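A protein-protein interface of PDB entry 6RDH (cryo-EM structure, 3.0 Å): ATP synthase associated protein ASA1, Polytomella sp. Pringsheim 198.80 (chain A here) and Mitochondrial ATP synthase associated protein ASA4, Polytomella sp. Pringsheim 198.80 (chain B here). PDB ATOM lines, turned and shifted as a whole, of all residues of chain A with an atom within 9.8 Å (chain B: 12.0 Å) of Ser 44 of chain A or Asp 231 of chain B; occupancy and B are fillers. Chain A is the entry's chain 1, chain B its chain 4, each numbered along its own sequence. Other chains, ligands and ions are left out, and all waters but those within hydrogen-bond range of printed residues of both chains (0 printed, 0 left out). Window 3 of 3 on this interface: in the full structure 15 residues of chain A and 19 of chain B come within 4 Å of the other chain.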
ATOM      1  N   ALA A  41     -13.217  26.085 -19.489  1.00  0.00           N
ATOM      2  CA  ALA A  41     -13.586  24.806 -20.072  1.00  0.00           C
ATOM      3  C   ALA A  41     -12.816  23.671 -19.416  1.00  0.00           C
ATOM      4  O   ALA A  41     -11.708  23.854 -18.911  1.00  0.00           O
ATOM      5  CB  ALA A  41     -13.337  24.805 -21.577  1.00  0.00           C
ATOM      6  N   SER A  42     -13.420  22.488 -19.438  1.00  0.00           N
ATOM      7  CA  SER A  42     -12.850  21.328 -18.773  1.00  0.00           C
ATOM      8  C   SER A  42     -11.649  20.796 -19.543  1.00  0.00           C
ATOM      9  O   SER A  42     -11.531  20.978 -20.757  1.00  0.00           O
ATOM     10  CB  SER A  42     -13.904  20.235 -18.627  1.00  0.00           C
ATOM     11  OG  SER A  42     -14.337  19.785 -19.897  1.00  0.00           O
ATOM     12  N   ALA A  43     -10.748  20.139 -18.821  1.00  0.00           N
ATOM     13  CA  ALA A  43      -9.529  19.631 -19.429  1.00  0.00           C
ATOM     14  C   ALA A  43      -9.830  18.413 -20.289  1.00  0.00           C
ATOM     15  O   ALA A  43     -10.524  17.489 -19.857  1.00  0.00           O
ATOM     16  CB  ALA A  43      -8.506  19.274 -18.355  1.00  0.00           C
ATOM     17  N   SER A  44      -9.313  18.420 -21.512  1.00  0.00           N
ATOM     18  CA  SER A  44      -9.464  17.284 -22.401  1.00  0.00           C
ATOM     19  C   SER A  44      -8.552  16.147 -21.965  1.00  0.00           C
ATOM     20  O   SER A  44      -7.576  16.338 -21.237  1.00  0.00           O
ATOM     21  CB  SER A  44      -9.134  17.677 -23.834  1.00  0.00           C
ATOM     22  OG  SER A  44      -7.776  18.059 -23.919  1.00  0.00           O
ATOM     23  N   ASN A  45      -8.879  14.948 -22.434  1.00  0.00           N
ATOM     24  CA  ASN A  45      -8.104  13.757 -22.133  1.00  0.00           C
ATOM     25  C   ASN A  45      -7.174  13.371 -23.274  1.00  0.00           C
ATOM     26  O   ASN A  45      -6.690  12.238 -23.307  1.00  0.00           O
ATOM     27  CB  ASN A  45      -9.043  12.600 -21.798  1.00  0.00           C
ATOM     28  CG  ASN A  45      -8.492  11.697 -20.720  1.00  0.00           C
ATOM     29  OD1 ASN A  45      -7.882  12.160 -19.760  1.00  0.00           O
ATOM     30  ND2 ASN A  45      -8.698  10.397 -20.876  1.00  0.00           N
ATOM     31  N   LEU A  46      -6.901  14.296 -24.199  1.00  0.00           N
ATOM     32  CA  LEU A  46      -6.125  13.962 -25.388  1.00  0.00           C
ATOM     33  C   LEU A  46      -4.664  13.704 -25.066  1.00  0.00           C
ATOM     34  O   LEU A  46      -4.033  12.873 -25.721  1.00  0.00           O
ATOM     35  CB  LEU A  46      -6.212  15.077 -26.417  1.00  0.00           C
ATOM     36  CG  LEU A  46      -5.775  14.708 -27.829  1.00  0.00           C
ATOM     37  CD1 LEU A  46      -6.948  14.143 -28.600  1.00  0.00           C
ATOM     38  CD2 LEU A  46      -5.165  15.886 -28.535  1.00  0.00           C
ATOM     39  N   VAL A  47      -4.102  14.400 -24.081  1.00  0.00           N
ATOM     40  CA  VAL A  47      -2.733  14.104 -23.680  1.00  0.00           C
ATOM     41  C   VAL A  47      -2.675  12.753 -22.986  1.00  0.00           C
ATOM     42  O   VAL A  47      -1.759  11.955 -23.216  1.00  0.00           O
ATOM     43  CB  VAL A  47      -2.188  15.222 -22.780  1.00  0.00           C
ATOM     44  CG1 VAL A  47      -0.752  14.945 -22.386  1.00  0.00           C
ATOM     45  CG2 VAL A  47      -2.310  16.554 -23.475  1.00  0.00           C
ATOM     46  N   ASN A  48      -3.688  12.449 -22.178  1.00  0.00           N
ATOM     47  CA  ASN A  48      -3.727  11.164 -21.496  1.00  0.00           C
ATOM     48  C   ASN A  48      -4.037  10.037 -22.469  1.00  0.00           C
ATOM     49  O   ASN A  48      -3.466   8.949 -22.361  1.00  0.00           O
ATOM     50  CB  ASN A  48      -4.754  11.204 -20.370  1.00  0.00           C
ATOM     51  CG  ASN A  48      -4.691   9.987 -19.484  1.00  0.00           C
ATOM     52  OD1 ASN A  48      -5.393   9.003 -19.709  1.00  0.00           O
ATOM     53  ND2 ASN A  48      -3.854  10.050 -18.457  1.00  0.00           N
ATOM     54  N   GLU A  49      -4.900  10.290 -23.456  1.00  0.00           N
ATOM     55  CA  GLU A  49      -5.171   9.275 -24.470  1.00  0.00           C
ATOM     56  C   GLU A  49      -3.982   9.058 -25.390  1.00  0.00           C
ATOM     57  O   GLU A  49      -3.756   7.936 -25.840  1.00  0.00           O
ATOM     58  CB  GLU A  49      -6.395   9.650 -25.288  1.00  0.00           C
ATOM     59  CG  GLU A  49      -7.689   9.267 -24.630  1.00  0.00           C
ATOM     60  CD  GLU A  49      -8.869   9.470 -25.544  1.00  0.00           C
ATOM     61  OE1 GLU A  49      -8.690  10.112 -26.598  1.00  0.00           O
ATOM     62  OE2 GLU A  49      -9.972   8.988 -25.211  1.00  0.00           O
ATOM     63  N   TRP A  50      -3.197  10.092 -25.666  1.00  0.00           N
ATOM     64  CA  TRP A  50      -2.033   9.875 -26.510  1.00  0.00           C
ATOM     65  C   TRP A  50      -0.904   9.206 -25.743  1.00  0.00           C
ATOM     66  O   TRP A  50      -0.148   8.423 -26.328  1.00  0.00           O
ATOM     67  CB  TRP A  50      -1.566  11.187 -27.121  1.00  0.00           C
ATOM     68  CG  TRP A  50      -2.398  11.641 -28.259  1.00  0.00           C
ATOM     69  CD1 TRP A  50      -3.656  11.234 -28.567  1.00  0.00           C
ATOM     70  CD2 TRP A  50      -2.038  12.601 -29.247  1.00  0.00           C
ATOM     71  NE1 TRP A  50      -4.103  11.877 -29.685  1.00  0.00           N
ATOM     72  CE2 TRP A  50      -3.124  12.724 -30.124  1.00  0.00           C
ATOM     73  CE3 TRP A  50      -0.898  13.365 -29.481  1.00  0.00           C
ATOM     74  CZ2 TRP A  50      -3.105  13.582 -31.209  1.00  0.00           C
ATOM     75  CZ3 TRP A  50      -0.884  14.215 -30.553  1.00  0.00           C
ATOM     76  CH2 TRP A  50      -1.977  14.319 -31.406  1.00  0.00           C
ATOM     77  N   LYS A  53      -2.010   5.627 -25.928  1.00  0.00           N
ATOM     78  CA  LYS A  53      -1.715   5.028 -27.219  1.00  0.00           C
ATOM     79  C   LYS A  53      -0.231   4.728 -27.360  1.00  0.00           C
ATOM     80  O   LYS A  53       0.144   3.691 -27.922  1.00  0.00           O
ATOM     81  CB  LYS A  53      -2.193   5.945 -28.332  1.00  0.00           C
ATOM     82  CG  LYS A  53      -3.679   5.964 -28.516  1.00  0.00           C
ATOM     83  CD  LYS A  53      -4.097   7.063 -29.455  1.00  0.00           C
ATOM     84  CE  LYS A  53      -5.595   7.065 -29.627  1.00  0.00           C
ATOM     85  NZ  LYS A  53      -6.030   8.058 -30.637  1.00  0.00           N
ATOM     86  N   LYS B 220      -7.434  32.709 -18.763  1.00  0.00           N
ATOM     87  CA  LYS B 220      -7.525  31.287 -18.452  1.00  0.00           C
ATOM     88  C   LYS B 220      -8.685  30.635 -19.180  1.00  0.00           C
ATOM     89  O   LYS B 220      -8.573  29.488 -19.619  1.00  0.00           O
ATOM     90  CB  LYS B 220      -7.660  31.072 -16.948  1.00  0.00           C
ATOM     91  CG  LYS B 220      -6.398  30.552 -16.298  1.00  0.00           C
ATOM     92  CD  LYS B 220      -5.242  31.507 -16.534  1.00  0.00           C
ATOM     93  CE  LYS B 220      -3.904  30.829 -16.360  1.00  0.00           C
ATOM     94  NZ  LYS B 220      -2.799  31.706 -16.835  1.00  0.00           N
ATOM     95  N   ALA B 221      -9.790  31.355 -19.354  1.00  0.00           N
ATOM     96  CA  ALA B 221     -10.884  30.780 -20.125  1.00  0.00           C
ATOM     97  C   ALA B 221     -10.557  30.699 -21.606  1.00  0.00           C
ATOM     98  O   ALA B 221     -10.976  29.749 -22.270  1.00  0.00           O
ATOM     99  CB  ALA B 221     -12.154  31.579 -19.930  1.00  0.00           C
ATOM    100  N   ILE B 222      -9.809  31.663 -22.142  1.00  0.00           N
ATOM    101  CA  ILE B 222      -9.430  31.566 -23.549  1.00  0.00           C
ATOM    102  C   ILE B 222      -8.391  30.468 -23.752  1.00  0.00           C
ATOM    103  O   ILE B 222      -8.420  29.760 -24.764  1.00  0.00           O
ATOM    104  CB  ILE B 222      -8.955  32.939 -24.057  1.00  0.00           C
ATOM    105  CG1 ILE B 222     -10.119  33.917 -24.039  1.00  0.00           C
ATOM    106  CG2 ILE B 222      -8.447  32.868 -25.468  1.00  0.00           C
ATOM    107  CD1 ILE B 222     -11.312  33.454 -24.831  1.00  0.00           C
ATOM    108  N   GLU B 223      -7.505  30.267 -22.777  1.00  0.00           N
ATOM    109  CA  GLU B 223      -6.556  29.161 -22.820  1.00  0.00           C
ATOM    110  C   GLU B 223      -7.268  27.821 -22.795  1.00  0.00           C
ATOM    111  O   GLU B 223      -6.939  26.916 -23.569  1.00  0.00           O
ATOM    112  CB  GLU B 223      -5.600  29.244 -21.637  1.00  0.00           C
ATOM    113  CG  GLU B 223      -4.450  30.171 -21.821  1.00  0.00           C
ATOM    114  CD  GLU B 223      -3.556  30.203 -20.616  1.00  0.00           C
ATOM    115  OE1 GLU B 223      -3.950  29.660 -19.570  1.00  0.00           O
ATOM    116  OE2 GLU B 223      -2.457  30.772 -20.708  1.00  0.00           O
ATOM    117  N   ALA B 224      -8.255  27.682 -21.911  1.00  0.00           N
ATOM    118  CA  ALA B 224      -9.004  26.438 -21.814  1.00  0.00           C
ATOM    119  C   ALA B 224      -9.844  26.192 -23.055  1.00  0.00           C
ATOM    120  O   ALA B 224      -9.952  25.052 -23.514  1.00  0.00           O
ATOM    121  CB  ALA B 224      -9.883  26.465 -20.574  1.00  0.00           C
ATOM    122  N   GLU B 225     -10.410  27.250 -23.637  1.00  0.00           N
ATOM    123  CA  GLU B 225     -11.192  27.094 -24.857  1.00  0.00           C
ATOM    124  C   GLU B 225     -10.311  26.708 -26.033  1.00  0.00           C
ATOM    125  O   GLU B 225     -10.682  25.836 -26.820  1.00  0.00           O
ATOM    126  CB  GLU B 225     -11.956  28.377 -25.169  1.00  0.00           C
ATOM    127  CG  GLU B 225     -12.700  28.346 -26.489  1.00  0.00           C
ATOM    128  CD  GLU B 225     -13.640  29.518 -26.666  1.00  0.00           C
ATOM    129  OE1 GLU B 225     -14.642  29.373 -27.397  1.00  0.00           O
ATOM    130  OE2 GLU B 225     -13.383  30.584 -26.071  1.00  0.00           O
ATOM    131  N   ALA B 226      -9.131  27.314 -26.151  1.00  0.00           N
ATOM    132  CA  ALA B 226      -8.243  26.979 -27.255  1.00  0.00           C
ATOM    133  C   ALA B 226      -7.675  25.578 -27.104  1.00  0.00           C
ATOM    134  O   ALA B 226      -7.544  24.857 -28.094  1.00  0.00           O
ATOM    135  CB  ALA B 226      -7.119  28.001 -27.361  1.00  0.00           C
ATOM    136  N   ALA B 227      -7.371  25.157 -25.875  1.00  0.00           N
ATOM    137  CA  ALA B 227      -6.883  23.800 -25.667  1.00  0.00           C
ATOM    138  C   ALA B 227      -7.967  22.768 -25.933  1.00  0.00           C
ATOM    139  O   ALA B 227      -7.697  21.723 -26.528  1.00  0.00           O
ATOM    140  CB  ALA B 227      -6.336  23.648 -24.253  1.00  0.00           C
ATOM    141  N   SER B 228      -9.206  23.060 -25.535  1.00  0.00           N
ATOM    142  CA  SER B 228     -10.309  22.150 -25.809  1.00  0.00           C
ATOM    143  C   SER B 228     -10.610  22.068 -27.297  1.00  0.00           C
ATOM    144  O   SER B 228     -10.866  20.981 -27.824  1.00  0.00           O
ATOM    145  CB  SER B 228     -11.543  22.603 -25.038  1.00  0.00           C
ATOM    146  OG  SER B 228     -12.647  21.771 -25.316  1.00  0.00           O
ATOM    147  N   ILE B 229     -10.535  23.200 -27.997  1.00  0.00           N
ATOM    148  CA  ILE B 229     -10.799  23.239 -29.431  1.00  0.00           C
ATOM    149  C   ILE B 229      -9.715  22.497 -30.200  1.00  0.00           C
ATOM    150  O   ILE B 229     -10.010  21.715 -31.113  1.00  0.00           O
ATOM    151  CB  ILE B 229     -10.937  24.707 -29.879  1.00  0.00           C
ATOM    152  CG1 ILE B 229     -12.344  25.210 -29.586  1.00  0.00           C
ATOM    153  CG2 ILE B 229     -10.658  24.878 -31.334  1.00  0.00           C
ATOM    154  CD1 ILE B 229     -12.553  26.645 -29.934  1.00  0.00           C
ATOM    155  N   LEU B 230      -8.454  22.690 -29.815  1.00  0.00           N
ATOM    156  CA  LEU B 230      -7.355  21.996 -30.471  1.00  0.00           C
ATOM    157  C   LEU B 230      -7.406  20.502 -30.213  1.00  0.00           C
ATOM    158  O   LEU B 230      -7.233  19.709 -31.141  1.00  0.00           O
ATOM    159  CB  LEU B 230      -6.022  22.554 -30.002  1.00  0.00           C
ATOM    160  CG  LEU B 230      -4.815  21.944 -30.689  1.00  0.00           C
ATOM    161  CD1 LEU B 230      -4.663  22.495 -32.070  1.00  0.00           C
ATOM    162  CD2 LEU B 230      -3.596  22.211 -29.897  1.00  0.00           C
ATOM    163  N   ASP B 231      -7.675  20.091 -28.974  1.00  0.00           N
ATOM    164  CA  ASP B 231      -7.728  18.669 -28.682  1.00  0.00           C
ATOM    165  C   ASP B 231      -8.969  17.997 -29.236  1.00  0.00           C
ATOM    166  O   ASP B 231      -8.987  16.773 -29.354  1.00  0.00           O
ATOM    167  CB  ASP B 231      -7.638  18.433 -27.181  1.00  0.00           C
ATOM    168  CG  ASP B 231      -6.320  18.897 -26.602  1.00  0.00           C
ATOM    169  OD1 ASP B 231      -6.251  19.116 -25.379  1.00  0.00           O
ATOM    170  OD2 ASP B 231      -5.355  19.068 -27.369  1.00  0.00           O
ATOM    171  N   ARG B 232     -10.009  18.751 -29.566  1.00  0.00           N
ATOM    172  CA  ARG B 232     -11.077  18.175 -30.368  1.00  0.00           C
ATOM    173  C   ARG B 232     -10.680  18.086 -31.827  1.00  0.00           C
ATOM    174  O   ARG B 232     -11.141  17.193 -32.537  1.00  0.00           O
ATOM    175  CB  ARG B 232     -12.348  19.007 -30.225  1.00  0.00           C
ATOM    176  CG  ARG B 232     -13.613  18.297 -30.627  1.00  0.00           C
ATOM    177  CD  ARG B 232     -14.811  19.208 -30.477  1.00  0.00           C
ATOM    178  NE  ARG B 232     -14.729  20.011 -29.262  1.00  0.00           N
ATOM    179  CZ  ARG B 232     -14.870  21.332 -29.224  1.00  0.00           C
ATOM    180  NH1 ARG B 232     -14.772  21.972 -28.070  1.00  0.00           N
ATOM    181  NH2 ARG B 232     -15.120  22.010 -30.335  1.00  0.00           N
ATOM    182  N   HIS B 233      -9.827  19.001 -32.283  1.00  0.00           N
ATOM    183  CA  HIS B 233      -9.421  19.046 -33.681  1.00  0.00           C
ATOM    184  C   HIS B 233      -8.284  18.081 -33.974  1.00  0.00           C
ATOM    185  O   HIS B 233      -8.206  17.546 -35.080  1.00  0.00           O
ATOM    186  CB  HIS B 233      -9.055  20.490 -34.032  1.00  0.00           C
ATOM    187  CG  HIS B 233      -8.092  20.649 -35.165  1.00  0.00           C
ATOM    188  ND1 HIS B 233      -6.728  20.605 -34.993  1.00  0.00           N
ATOM    189  CD2 HIS B 233      -8.295  20.946 -36.466  1.00  0.00           C
ATOM    190  CE1 HIS B 233      -6.132  20.816 -36.151  1.00  0.00           C
ATOM    191  NE2 HIS B 233      -7.062  21.026 -37.061  1.00  0.00           N
ATOM    192  N   LEU B 234      -7.418  17.815 -32.998  1.00  0.00           N
ATOM    193  CA  LEU B 234      -6.307  16.896 -33.211  1.00  0.00           C
ATOM    194  C   LEU B 234      -6.729  15.436 -33.225  1.00  0.00           C
ATOM    195  O   LEU B 234      -5.889  14.575 -33.489  1.00  0.00           O
ATOM    196  CB  LEU B 234      -5.246  17.090 -32.137  1.00  0.00           C
ATOM    197  CG  LEU B 234      -4.386  18.338 -32.228  1.00  0.00           C
ATOM    198  CD1 LEU B 234      -3.271  18.229 -31.250  1.00  0.00           C
ATOM    199  CD2 LEU B 234      -3.842  18.521 -33.610  1.00  0.00           C
ATOM    200  N   ALA B 235      -7.985  15.132 -32.933  1.00  0.00           N
ATOM    201  CA  ALA B 235      -8.481  13.769 -32.994  1.00  0.00           C
ATOM    202  C   ALA B 235      -9.088  13.420 -34.341  1.00  0.00           C
ATOM    203  O   ALA B 235      -9.448  12.262 -34.556  1.00  0.00           O
ATOM    204  CB  ALA B 235      -9.516  13.542 -31.899  1.00  0.00           C
ATOM    205  N   LYS B 236      -9.214  14.339 -35.204  1.00  0.00           N
ATOM    206  CA  LYS B 236      -9.764  14.087 -36.522  1.00  0.00           C
ATOM    207  C   LYS B 236      -8.662  13.687 -37.495  1.00  0.00           C
ATOM    208  O   LYS B 236      -7.498  14.033 -37.295  1.00  0.00           O
ATOM    209  CB  LYS B 236     -10.464  15.330 -37.047  1.00  0.00           C
ATOM    210  CG  LYS B 236     -11.430  15.955 -36.079  1.00  0.00           C
ATOM    211  CD  LYS B 236     -12.095  17.161 -36.700  1.00  0.00           C
ATOM    212  CE  LYS B 236     -12.875  17.943 -35.675  1.00  0.00           C
ATOM    213  NZ  LYS B 236     -13.864  17.090 -34.982  1.00  0.00           N
ATOM    214  N   PRO B 237      -8.979  12.949 -38.553  1.00  0.00           N
ATOM    215  CA  PRO B 237      -8.017  12.784 -39.642  1.00  0.00           C
ATOM    216  C   PRO B 237      -7.899  14.071 -40.434  1.00  0.00           C
ATOM    217  O   PRO B 237      -8.699  14.992 -40.298  1.00  0.00           O
ATOM    218  CB  PRO B 237      -8.619  11.662 -40.482  1.00  0.00           C
ATOM    219  CG  PRO B 237     -10.050  11.699 -40.168  1.00  0.00           C
ATOM    220  CD  PRO B 237     -10.146  12.077 -38.736  1.00  0.00           C
ATOM    221  N   GLN B 240     -10.800  15.187 -43.022  1.00  0.00           N
ATOM    222  CA  GLN B 240     -11.976  15.759 -42.380  1.00  0.00           C
ATOM    223  C   GLN B 240     -11.728  17.199 -41.972  1.00  0.00           C
ATOM    224  O   GLN B 240     -12.602  18.054 -42.144  1.00  0.00           O
ATOM    225  CB  GLN B 240     -12.365  14.925 -41.164  1.00  0.00           C
ATOM    226  CG  GLN B 240     -13.575  15.440 -40.430  1.00  0.00           C
ATOM    227  CD  GLN B 240     -13.788  14.748 -39.107  1.00  0.00           C
ATOM    228  OE1 GLN B 240     -14.557  15.211 -38.268  1.00  0.00           O
ATOM    229  NE2 GLN B 240     -13.113  13.626 -38.913  1.00  0.00           N
ATOM    230  N   ILE B 241     -10.529  17.483 -41.459  1.00  0.00           N
ATOM    231  CA  ILE B 241     -10.152  18.839 -41.068  1.00  0.00           C
ATOM    232  C   ILE B 241     -10.128  19.755 -42.275  1.00  0.00           C
ATOM    233  O   ILE B 241     -10.666  20.869 -42.237  1.00  0.00           O
ATOM    234  CB  ILE B 241      -8.791  18.814 -40.357  1.00  0.00           C
ATOM    235  CG1 ILE B 241      -8.932  18.189 -38.987  1.00  0.00           C
ATOM    236  CG2 ILE B 241      -8.207  20.188 -40.235  1.00  0.00           C
ATOM    237  CD1 ILE B 241      -7.637  17.901 -38.374  1.00  0.00           C
ATOM    238  N   GLU B 244     -13.774  20.264 -43.580  1.00  0.00           N
ATOM    239  CA  GLU B 244     -14.562  21.065 -42.649  1.00  0.00           C
ATOM    240  C   GLU B 244     -14.156  22.528 -42.705  1.00  0.00           C
ATOM    241  O   GLU B 244     -15.015  23.415 -42.768  1.00  0.00           O
ATOM    242  CB  GLU B 244     -14.400  20.531 -41.229  1.00  0.00           C
ATOM    243  CG  GLU B 244     -15.342  19.406 -40.849  1.00  0.00           C
ATOM    244  CD  GLU B 244     -15.175  18.974 -39.399  1.00  0.00           C
ATOM    245  OE1 GLU B 244     -14.170  19.366 -38.769  1.00  0.00           O
ATOM    246  OE2 GLU B 244     -16.053  18.245 -38.888  1.00  0.00           O
ATOM    247  N   GLN B 245     -12.850  22.797 -42.723  1.00  0.00           N
ATOM    248  CA  GLN B 245     -12.388  24.173 -42.785  1.00  0.00           C
ATOM    249  C   GLN B 245     -12.654  24.805 -44.140  1.00  0.00           C
ATOM    250  O   GLN B 245     -12.957  26.000 -44.208  1.00  0.00           O
ATOM    251  CB  GLN B 245     -10.906  24.235 -42.455  1.00  0.00           C
ATOM    252  CG  GLN B 245     -10.603  23.943 -41.017  1.00  0.00           C
ATOM    253  CD  GLN B 245      -9.238  24.412 -40.637  1.00  0.00           C
ATOM    254  OE1 GLN B 245      -8.420  24.710 -41.499  1.00  0.00           O
ATOM    255  NE2 GLN B 245      -8.980  24.502 -39.345  1.00  0.00           N
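Of the printed residues of chain B, Ala 41 of chain A touches Ala 224.
No residue of chain B comes within 4 Å of Asn 45 of chain A.
Leu 46 of chain A touches just these residues of chain B: Asp 231 and Leu 234.
No residue of chain B comes within 4 Å of Val 47 of chain A.
Of the printed residues of chain B, Trp 50 of chain A touches Leu 234 (3.7 Å).
Lys 220 of chain B touches none of the printed residues of chain A.
Printed residues of chain A within 4 Å of Ala 224 of chain B: Ala 41.
No residue of chain A comes within 4 Å of Ser 228 of chain B.
Leu 230 of chain B touches none of the printed residues of chain A.
Asp 231 of chain B touches two residues of chain A.
Of the printed residues of chain A, Leu 234 of chain B touches Leu 46 and Trp 50.
Gln 240 of chain B touches none of the printed residues of chain A.
The nearest residue of chain A that does not touch Asp 231 of chain B is Val 47 of chain A (5.1 Å).
The nearest printed residue of chain A that does not touch Ala 224 of chain B is Ser 42 of chain A (5.2 Å).
Printed residues of chain B that touch a printed residue of chain A: Ala 224, Asp 231 and Leu 234.
Along chain B the printed residues that touch a printed residue of chain A span positions 224 to 234.
Among the printed residues, 5 pairs touch across the chains.
Among the printed residues, no Asp or Glu carboxylate lies within 4 Å of a Lys or Arg side-chain nitrogen of the other chain.
The side-chain hydroxyl (OG) of Ser 44 of chain A lies close to the side-chain carboxylate (OD1) of Asp 231 of chain B (2.4 Å).
Ala 224 of chain B touches Ala 41 of chain A (CB to N, 3.5 Å).
Asp 231 of chain B touches Leu 46 of chain A.
CD2 of Leu 46 of chain A touches CB of Leu 234 of chain B, at 3.8 Å.
Leu 234 of chain B touches Trp 50 of chain A.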
